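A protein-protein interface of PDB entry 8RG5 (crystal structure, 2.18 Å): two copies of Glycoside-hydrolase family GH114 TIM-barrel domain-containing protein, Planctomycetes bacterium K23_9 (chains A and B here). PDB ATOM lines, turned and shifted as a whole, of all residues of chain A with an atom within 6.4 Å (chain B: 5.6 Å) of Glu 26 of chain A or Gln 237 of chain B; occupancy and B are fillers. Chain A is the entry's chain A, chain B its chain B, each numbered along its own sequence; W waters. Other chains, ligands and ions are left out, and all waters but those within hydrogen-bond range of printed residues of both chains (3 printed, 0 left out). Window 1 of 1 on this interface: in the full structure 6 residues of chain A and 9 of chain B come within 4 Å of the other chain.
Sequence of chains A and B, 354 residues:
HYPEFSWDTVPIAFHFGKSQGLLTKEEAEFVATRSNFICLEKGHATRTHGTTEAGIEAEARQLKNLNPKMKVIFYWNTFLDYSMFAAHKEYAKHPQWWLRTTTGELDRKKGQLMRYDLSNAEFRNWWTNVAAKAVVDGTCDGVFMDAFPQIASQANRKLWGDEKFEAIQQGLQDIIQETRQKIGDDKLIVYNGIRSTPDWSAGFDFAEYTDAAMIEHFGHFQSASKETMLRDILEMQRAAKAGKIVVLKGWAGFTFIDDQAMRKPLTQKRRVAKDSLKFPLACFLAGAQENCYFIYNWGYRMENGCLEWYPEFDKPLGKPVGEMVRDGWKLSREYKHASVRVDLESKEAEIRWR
Of chain A, only Glu 26 (3.8 Å) comes within 4 Å of Gln 237 of chain B. Printed residues of chain A within 4 Å of Met 324 of chain B: Glu 26 (3.9 Å). Printed residues of chain B within 4 Å of Lys 25 of chain A: Arg 326. Printed residues of chain A within 4 Å of Glu 323 of chain B: Thr 24. Of the printed residues of chain B, Thr 24 of chain A touches Glu 323. Of the printed residues of chain A, Leu 234 of chain B touches Glu 26. Gly 287 of chain B touches none of the printed residues of chain A. The nearest printed residue of chain B that does not touch Glu 26 of chain A is Glu 323 of chain B (6.4 Å).
N of Glu 26 of chain A sits close to OG1 of Thr 24 of chain A. The backbone NH of Glu 27 of chain A is in hydrogen-bond range of the side-chain hydroxyl of Thr 24 of chain A (2.9 Å). OE1 of Glu 323 of chain B lies within salt-bridge range of NZ of Lys 241 of chain B (2.7 Å).
Glu 323 of chain B touches Thr 24 of chain A (CB to CG2, 3.99 Å). NH2 of Arg 326 of chain B touches CD of Lys 25 of chain A, at 3.2 Å. Glu 26 of chain A touches Leu 234 of chain B (CG to CD2, 3.6 Å). OE1 of Gln 237 of chain B touches CG of Glu 26 of chain A (3.8 Å). Glu 26 of chain A touches Met 324 of chain B.
Water W3 lies within hydrogen-bond range of the side-chain carboxylate (OE2) of Glu 27 of chain A (2.5 Å) and the side-chain amino group (NZ) of Lys 241 of chain B (3.3 Å). Water W2 lies within hydrogen-bond range of the side-chain carboxylate (OE1) of Glu 26 of chain A (2.5 Å), the backbone carbonyl oxygen (O) of Met 324 of chain B (2.8 Å) and the side-chain amide nitrogen (NE2) of Gln 237 of chain B (2.9 Å). Water W1 bridges OG1 of Thr 24 of chain A (2.6 Å) and OE1 of Glu 323 of chain B (3.4 Å).
No position is printed for both chains.
The guanidinium group (NE) of Arg 326 of chain B is in salt-bridge range of the side-chain carboxylate (OE2) of Glu 26 of chain A (2.8 Å). The side-chain carboxylate of Glu 29 of chain A is in salt-bridge range of the guanidinium group of Arg 326 of chain B.
Hydrophobic or aromatic side chains of chain B that line the printed part of chain A: Leu 234. Of the 9 printed residues of chain A, 4 touch a printed residue of chain B. Along chain A the printed residues that touch a printed residue of chain B span positions 24 to 29. Among the printed residues, 7 pairs touch across the chains. Among the printed residues, Asp or Glu carboxylates within 4 Å of a Lys or Arg side-chain nitrogen of the other chain: Glu 26 of chain A with Arg 326 of chain B and Glu 29 of chain A with Arg 326 of chain B.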
ATOM      1  N   LEU A  23     -25.251 -34.810 -29.338  1.00  0.00           N
ATOM      2  CA  LEU A  23     -24.782 -33.436 -29.445  1.00  0.00           C
ATOM      3  C   LEU A  23     -25.193 -32.686 -28.177  1.00  0.00           C
ATOM      4  O   LEU A  23     -26.302 -32.894 -27.662  1.00  0.00           O
ATOM      5  CB  LEU A  23     -25.387 -32.745 -30.662  1.00  0.00           C
ATOM      6  CG  LEU A  23     -25.094 -33.299 -32.056  1.00  0.00           C
ATOM      7  CD1 LEU A  23     -25.825 -32.450 -33.099  1.00  0.00           C
ATOM      8  CD2 LEU A  23     -23.604 -33.303 -32.287  1.00  0.00           C
ATOM      9  N   THR A  24     -24.307 -31.829 -27.660  1.00  0.00           N
ATOM     10  CA  THR A  24     -24.767 -30.921 -26.610  1.00  0.00           C
ATOM     11  C   THR A  24     -25.895 -30.051 -27.184  1.00  0.00           C
ATOM     12  O   THR A  24     -26.079 -29.929 -28.391  1.00  0.00           O
ATOM     13  CB  THR A  24     -23.657 -29.993 -26.102  1.00  0.00           C
ATOM     14  OG1 THR A  24     -23.192 -29.197 -27.207  1.00  0.00           O
ATOM     15  CG2 THR A  24     -22.529 -30.800 -25.446  1.00  0.00           C
ATOM     16  N   LYS A  25     -26.610 -29.376 -26.299  1.00  0.00           N
ATOM     17  CA  LYS A  25     -27.592 -28.391 -26.752  1.00  0.00           C
ATOM     18  C   LYS A  25     -26.947 -27.344 -27.663  1.00  0.00           C
ATOM     19  O   LYS A  25     -27.504 -26.986 -28.704  1.00  0.00           O
ATOM     20  CB  LYS A  25     -28.238 -27.757 -25.511  1.00  0.00           C
ATOM     21  CG  LYS A  25     -28.953 -26.450 -25.767  1.00  0.00           C
ATOM     22  CD  LYS A  25     -29.704 -25.899 -24.521  1.00  0.00           C
ATOM     23  CE  LYS A  25     -30.515 -26.942 -23.754  1.00  0.00           C
ATOM     24  NZ  LYS A  25     -31.895 -27.096 -24.303  1.00  0.00           N
ATOM     25  N   GLU A  26     -25.762 -26.846 -27.292  1.00  0.00           N
ATOM     26  CA  GLU A  26     -25.082 -25.845 -28.101  1.00  0.00           C
ATOM     27  C   GLU A  26     -24.666 -26.433 -29.428  1.00  0.00           C
ATOM     28  O   GLU A  26     -24.812 -25.791 -30.472  1.00  0.00           O
ATOM     29  CB  GLU A  26     -23.872 -25.272 -27.344  1.00  0.00           C
ATOM     30  CG  GLU A  26     -24.240 -24.370 -26.149  1.00  0.00           C
ATOM     31  CD  GLU A  26     -24.967 -25.124 -25.026  1.00  0.00           C
ATOM     32  OE1 GLU A  26     -24.526 -26.236 -24.619  1.00  0.00           O
ATOM     33  OE2 GLU A  26     -25.980 -24.581 -24.526  1.00  0.00           O
ATOM     34  N   GLU A  27     -24.205 -27.692 -29.433  1.00  0.00           N
ATOM     35  CA  GLU A  27     -23.839 -28.306 -30.708  1.00  0.00           C
ATOM     36  C   GLU A  27     -25.070 -28.534 -31.588  1.00  0.00           C
ATOM     37  O   GLU A  27     -25.014 -28.338 -32.821  1.00  0.00           O
ATOM     38  CB  GLU A  27     -23.083 -29.619 -30.478  1.00  0.00           C
ATOM     39  CG  GLU A  27     -21.656 -29.398 -29.877  1.00  0.00           C
ATOM     40  CD  GLU A  27     -21.062 -30.679 -29.235  1.00  0.00           C
ATOM     41  OE1 GLU A  27     -21.791 -31.681 -29.071  1.00  0.00           O
ATOM     42  OE2 GLU A  27     -19.858 -30.673 -28.911  1.00  0.00           O
ATOM     43  N   ALA A  28     -26.181 -28.961 -30.981  1.00  0.00           N
ATOM     44  CA  ALA A  28     -27.393 -29.215 -31.761  1.00  0.00           C
ATOM     45  C   ALA A  28     -27.959 -27.913 -32.329  1.00  0.00           C
ATOM     46  O   ALA A  28     -28.392 -27.862 -33.490  1.00  0.00           O
ATOM     47  CB  ALA A  28     -28.433 -29.909 -30.877  1.00  0.00           C
ATOM     48  N   GLU A  29     -27.970 -26.851 -31.520  1.00  0.00           N
ATOM     49  CA  GLU A  29     -28.368 -25.545 -32.029  1.00  0.00           C
ATOM     50  C   GLU A  29     -27.445 -25.105 -33.169  1.00  0.00           C
ATOM     51  O   GLU A  29     -27.903 -24.586 -34.196  1.00  0.00           O
ATOM     52  CB  GLU A  29     -28.334 -24.496 -30.908  1.00  0.00           C
ATOM     53  CG  GLU A  29     -29.626 -24.276 -30.212  1.00  0.00           C
ATOM     54  CD  GLU A  29     -29.481 -23.382 -28.972  1.00  0.00           C
ATOM     55  OE1 GLU A  29     -28.655 -22.450 -28.999  1.00  0.00           O
ATOM     56  OE2 GLU A  29     -30.196 -23.623 -27.982  1.00  0.00           O
ATOM     57  N   PHE A  30     -26.133 -25.251 -32.983  1.00  0.00           N
ATOM     58  CA  PHE A  30     -25.200 -24.839 -34.029  1.00  0.00           C
ATOM     59  C   PHE A  30     -25.547 -25.525 -35.346  1.00  0.00           C
ATOM     60  O   PHE A  30     -25.686 -24.883 -36.388  1.00  0.00           O
ATOM     61  CB  PHE A  30     -23.768 -25.161 -33.619  1.00  0.00           C
ATOM     62  CG  PHE A  30     -22.761 -24.908 -34.700  1.00  0.00           C
ATOM     63  CD1 PHE A  30     -22.491 -25.857 -35.662  1.00  0.00           C
ATOM     64  CD2 PHE A  30     -22.099 -23.698 -34.762  1.00  0.00           C
ATOM     65  CE1 PHE A  30     -21.581 -25.615 -36.669  1.00  0.00           C
ATOM     66  CE2 PHE A  30     -21.160 -23.453 -35.741  1.00  0.00           C
ATOM     67  CZ  PHE A  30     -20.905 -24.393 -36.700  1.00  0.00           C
ATOM     68  N   VAL A  31     -25.750 -26.839 -35.298  1.00  0.00           N
ATOM     69  CA  VAL A  31     -26.070 -27.618 -36.498  1.00  0.00           C
ATOM     70  C   VAL A  31     -27.467 -27.262 -37.046  1.00  0.00           C
ATOM     71  O   VAL A  31     -27.636 -26.990 -38.254  1.00  0.00           O
ATOM     72  CB  VAL A  31     -25.932 -29.123 -36.161  1.00  0.00           C
ATOM     73  CG1 VAL A  31     -26.625 -29.962 -37.164  1.00  0.00           C
ATOM     74  CG2 VAL A  31     -24.461 -29.512 -36.071  1.00  0.00           C
ATOM     75  N   ASP B 232     -23.418 -13.565 -24.372  1.00  0.00           N
ATOM     76  CA  ASP B 232     -21.970 -13.368 -24.246  1.00  0.00           C
ATOM     77  C   ASP B 232     -21.259 -14.681 -23.931  1.00  0.00           C
ATOM     78  O   ASP B 232     -20.258 -15.033 -24.579  1.00  0.00           O
ATOM     79  CB  ASP B 232     -21.665 -12.305 -23.180  1.00  0.00           C
ATOM     80  CG  ASP B 232     -21.889 -10.867 -23.708  1.00  0.00           C
ATOM     81  OD1 ASP B 232     -21.870 -10.651 -24.934  1.00  0.00           O
ATOM     82  OD2 ASP B 232     -22.050  -9.945 -22.882  1.00  0.00           O
ATOM     83  N   ILE B 233     -21.797 -15.454 -22.978  1.00  0.00           N
ATOM     84  CA  ILE B 233     -21.156 -16.713 -22.573  1.00  0.00           C
ATOM     85  C   ILE B 233     -21.167 -17.714 -23.722  1.00  0.00           C
ATOM     86  O   ILE B 233     -20.165 -18.382 -23.998  1.00  0.00           O
ATOM     87  CB  ILE B 233     -21.866 -17.286 -21.330  1.00  0.00           C
ATOM     88  CG1 ILE B 233     -21.696 -16.352 -20.134  1.00  0.00           C
ATOM     89  CG2 ILE B 233     -21.321 -18.654 -20.924  1.00  0.00           C
ATOM     90  CD1 ILE B 233     -22.684 -16.636 -18.939  1.00  0.00           C
ATOM     91  N   LEU B 234     -22.313 -17.857 -24.394  1.00  0.00           N
ATOM     92  CA  LEU B 234     -22.402 -18.773 -25.533  1.00  0.00           C
ATOM     93  C   LEU B 234     -21.453 -18.369 -26.650  1.00  0.00           C
ATOM     94  O   LEU B 234     -20.870 -19.226 -27.326  1.00  0.00           O
ATOM     95  CB  LEU B 234     -23.827 -18.803 -26.066  1.00  0.00           C
ATOM     96  CG  LEU B 234     -24.873 -19.537 -25.216  1.00  0.00           C
ATOM     97  CD1 LEU B 234     -26.266 -19.419 -25.848  1.00  0.00           C
ATOM     98  CD2 LEU B 234     -24.492 -20.996 -25.053  1.00  0.00           C
ATOM     99  N   GLU B 235     -21.271 -17.070 -26.865  1.00  0.00           N
ATOM    100  CA  GLU B 235     -20.377 -16.656 -27.939  1.00  0.00           C
ATOM    101  C   GLU B 235     -18.912 -16.860 -27.546  1.00  0.00           C
ATOM    102  O   GLU B 235     -18.087 -17.221 -28.402  1.00  0.00           O
ATOM    103  CB  GLU B 235     -20.678 -15.203 -28.319  1.00  0.00           C
ATOM    104  CG  GLU B 235     -19.867 -14.636 -29.465  1.00  0.00           C
ATOM    105  CD  GLU B 235     -19.946 -15.445 -30.753  1.00  0.00           C
ATOM    106  OE1 GLU B 235     -20.807 -16.352 -30.890  1.00  0.00           O
ATOM    107  OE2 GLU B 235     -19.131 -15.153 -31.645  1.00  0.00           O
ATOM    108  N   MET B 236     -18.568 -16.665 -26.268  1.00  0.00           N
ATOM    109  CA  MET B 236     -17.214 -16.997 -25.807  1.00  0.00           C
ATOM    110  C   MET B 236     -16.916 -18.456 -26.127  1.00  0.00           C
ATOM    111  O   MET B 236     -15.917 -18.777 -26.775  1.00  0.00           O
ATOM    112  CB  MET B 236     -17.055 -16.753 -24.292  1.00  0.00           C
ATOM    113  CG  MET B 236     -15.678 -17.201 -23.765  1.00  0.00           C
ATOM    114  SD  MET B 236     -15.334 -16.921 -22.019  1.00  0.00           S
ATOM    115  CE  MET B 236     -16.783 -17.601 -21.277  1.00  0.00           C
ATOM    116  N   GLN B 237     -17.830 -19.340 -25.712  1.00  0.00           N
ATOM    117  CA  GLN B 237     -17.654 -20.775 -25.877  1.00  0.00           C
ATOM    118  C   GLN B 237     -17.510 -21.156 -27.350  1.00  0.00           C
ATOM    119  O   GLN B 237     -16.628 -21.934 -27.711  1.00  0.00           O
ATOM    120  CB  GLN B 237     -18.844 -21.499 -25.227  1.00  0.00           C
ATOM    121  CG  GLN B 237     -18.707 -22.969 -25.372  1.00  0.00           C
ATOM    122  CD  GLN B 237     -19.994 -23.643 -25.691  1.00  0.00           C
ATOM    123  OE1 GLN B 237     -20.631 -23.320 -26.710  1.00  0.00           O
ATOM    124  NE2 GLN B 237     -20.387 -24.617 -24.831  1.00  0.00           N
ATOM    125  N   ARG B 238     -18.389 -20.656 -28.214  1.00  0.00           N
ATOM    126  CA  ARG B 238     -18.300 -21.009 -29.627  1.00  0.00           C
ATOM    127  C   ARG B 238     -16.982 -20.513 -30.231  1.00  0.00           C
ATOM    128  O   ARG B 238     -16.263 -21.265 -30.913  1.00  0.00           O
ATOM    129  CB  ARG B 238     -19.496 -20.439 -30.401  1.00  0.00           C
ATOM    130  CG  ARG B 238     -19.529 -20.866 -31.893  1.00  0.00           C
ATOM    131  CD  ARG B 238     -20.388 -19.885 -32.711  1.00  0.00           C
ATOM    132  NE  ARG B 238     -19.746 -18.585 -32.771  1.00  0.00           N
ATOM    133  CZ  ARG B 238     -18.704 -18.295 -33.540  1.00  0.00           C
ATOM    134  NH1 ARG B 238     -18.223 -19.173 -34.400  1.00  0.00           N
ATOM    135  NH2 ARG B 238     -18.102 -17.112 -33.404  1.00  0.00           N
ATOM    136  N   ALA B 239     -16.642 -19.249 -29.981  1.00  0.00           N
ATOM    137  CA  ALA B 239     -15.470 -18.674 -30.629  1.00  0.00           C
ATOM    138  C   ALA B 239     -14.184 -19.337 -30.147  1.00  0.00           C
ATOM    139  O   ALA B 239     -13.228 -19.502 -30.920  1.00  0.00           O
ATOM    140  CB  ALA B 239     -15.391 -17.172 -30.375  1.00  0.00           C
ATOM    141  N   ALA B 240     -14.126 -19.683 -28.863  1.00  0.00           N
ATOM    142  CA  ALA B 240     -12.932 -20.334 -28.334  1.00  0.00           C
ATOM    143  C   ALA B 240     -12.860 -21.782 -28.806  1.00  0.00           C
ATOM    144  O   ALA B 240     -11.765 -22.307 -29.074  1.00  0.00           O
ATOM    145  CB  ALA B 240     -12.934 -20.227 -26.808  1.00  0.00           C
ATOM    146  N   LYS B 241     -14.020 -22.451 -28.947  1.00  0.00           N
ATOM    147  CA  LYS B 241     -13.998 -23.773 -29.559  1.00  0.00           C
ATOM    148  C   LYS B 241     -13.563 -23.691 -31.015  1.00  0.00           C
ATOM    149  O   LYS B 241     -12.978 -24.639 -31.544  1.00  0.00           O
ATOM    150  CB  LYS B 241     -15.364 -24.451 -29.475  1.00  0.00           C
ATOM    151  CG  LYS B 241     -15.674 -25.076 -28.129  1.00  0.00           C
ATOM    152  CD  LYS B 241     -17.147 -25.543 -28.042  1.00  0.00           C
ATOM    153  CE  LYS B 241     -17.443 -26.223 -26.692  1.00  0.00           C
ATOM    154  NZ  LYS B 241     -16.804 -27.515 -26.646  1.00  0.00           N
ATOM    155  N   ALA B 242     -13.852 -22.590 -31.680  1.00  0.00           N
ATOM    156  CA  ALA B 242     -13.418 -22.422 -33.058  1.00  0.00           C
ATOM    157  C   ALA B 242     -11.930 -22.084 -33.162  1.00  0.00           C
ATOM    158  O   ALA B 242     -11.411 -21.966 -34.280  1.00  0.00           O
ATOM    159  CB  ALA B 242     -14.264 -21.326 -33.735  1.00  0.00           C
ATOM    160  N   GLY B 287     -18.518 -21.191 -19.139  1.00  0.00           N
ATOM    161  CA  GLY B 287     -18.353 -21.288 -20.573  1.00  0.00           C
ATOM    162  C   GLY B 287     -16.928 -21.344 -21.084  1.00  0.00           C
ATOM    163  O   GLY B 287     -16.701 -21.540 -22.278  1.00  0.00           O
ATOM    164  N   GLN B 289     -13.199 -21.927 -22.356  1.00  0.00           N
ATOM    165  CA  GLN B 289     -12.519 -22.953 -23.144  1.00  0.00           C
ATOM    166  C   GLN B 289     -11.051 -22.561 -23.179  1.00  0.00           C
ATOM    167  O   GLN B 289     -10.654 -21.526 -22.614  1.00  0.00           O
ATOM    168  CB  GLN B 289     -13.133 -23.065 -24.546  1.00  0.00           C
ATOM    169  CG  GLN B 289     -14.673 -23.075 -24.579  1.00  0.00           C
ATOM    170  CD  GLN B 289     -15.297 -24.369 -24.050  1.00  0.00           C
ATOM    171  OE1 GLN B 289     -16.393 -24.390 -23.469  1.00  0.00           O
ATOM    172  NE2 GLN B 289     -14.613 -25.453 -24.285  1.00  0.00           N
ATOM    173  N   GLU B 323     -18.560 -30.753 -20.684  1.00  0.00           N
ATOM    174  CA  GLU B 323     -19.052 -29.579 -21.396  1.00  0.00           C
ATOM    175  C   GLU B 323     -19.981 -28.761 -20.510  1.00  0.00           C
ATOM    176  O   GLU B 323     -20.603 -29.283 -19.582  1.00  0.00           O
ATOM    177  CB  GLU B 323     -19.776 -30.026 -22.666  1.00  0.00           C
ATOM    178  CG  GLU B 323     -18.874 -30.823 -23.630  1.00  0.00           C
ATOM    179  CD  GLU B 323     -17.848 -29.925 -24.341  1.00  0.00           C
ATOM    180  OE1 GLU B 323     -18.242 -28.830 -24.798  1.00  0.00           O
ATOM    181  OE2 GLU B 323     -16.668 -30.303 -24.424  1.00  0.00           O
ATOM    182  N   MET B 324     -20.073 -27.467 -20.800  1.00  0.00           N
ATOM    183  CA  MET B 324     -21.107 -26.652 -20.190  1.00  0.00           C
ATOM    184  C   MET B 324     -22.452 -27.334 -20.344  1.00  0.00           C
ATOM    185  O   MET B 324     -22.815 -27.769 -21.445  1.00  0.00           O
ATOM    186  CB  MET B 324     -21.178 -25.267 -20.838  1.00  0.00           C
ATOM    187  CG  MET B 324     -21.800 -24.224 -19.925  1.00  0.00           C
ATOM    188  SD  MET B 324     -21.949 -22.591 -20.654  1.00  0.00           S
ATOM    189  CE  MET B 324     -22.829 -22.930 -22.157  1.00  0.00           C
ATOM    190  N   ARG B 326     -26.490 -26.521 -19.771  1.00  0.00           N
ATOM    191  CA  ARG B 326     -27.427 -25.421 -19.629  1.00  0.00           C
ATOM    192  C   ARG B 326     -28.842 -25.970 -19.488  1.00  0.00           C
ATOM    193  O   ARG B 326     -29.297 -26.753 -20.324  1.00  0.00           O
ATOM    194  CB  ARG B 326     -27.347 -24.480 -20.844  1.00  0.00           C
ATOM    195  CG  ARG B 326     -28.558 -23.503 -20.987  1.00  0.00           C
ATOM    196  CD  ARG B 326     -28.285 -22.397 -22.047  1.00  0.00           C
ATOM    197  NE  ARG B 326     -27.956 -22.904 -23.393  1.00  0.00           N
ATOM    198  CZ  ARG B 326     -28.742 -22.768 -24.453  1.00  0.00           C
ATOM    199  NH1 ARG B 326     -29.916 -22.168 -24.368  1.00  0.00           N
ATOM    200  NH2 ARG B 326     -28.336 -23.226 -25.633  1.00  0.00           N
HETATM  201  O   HOH W   1     -21.095 -27.869 -26.450  1.00  0.00           O
HETATM  202  O   HOH W   2     -22.134 -26.741 -24.013  1.00  0.00           O
HETATM  203  O   HOH W   3     -18.182 -28.861 -29.381  1.00  0.00           O
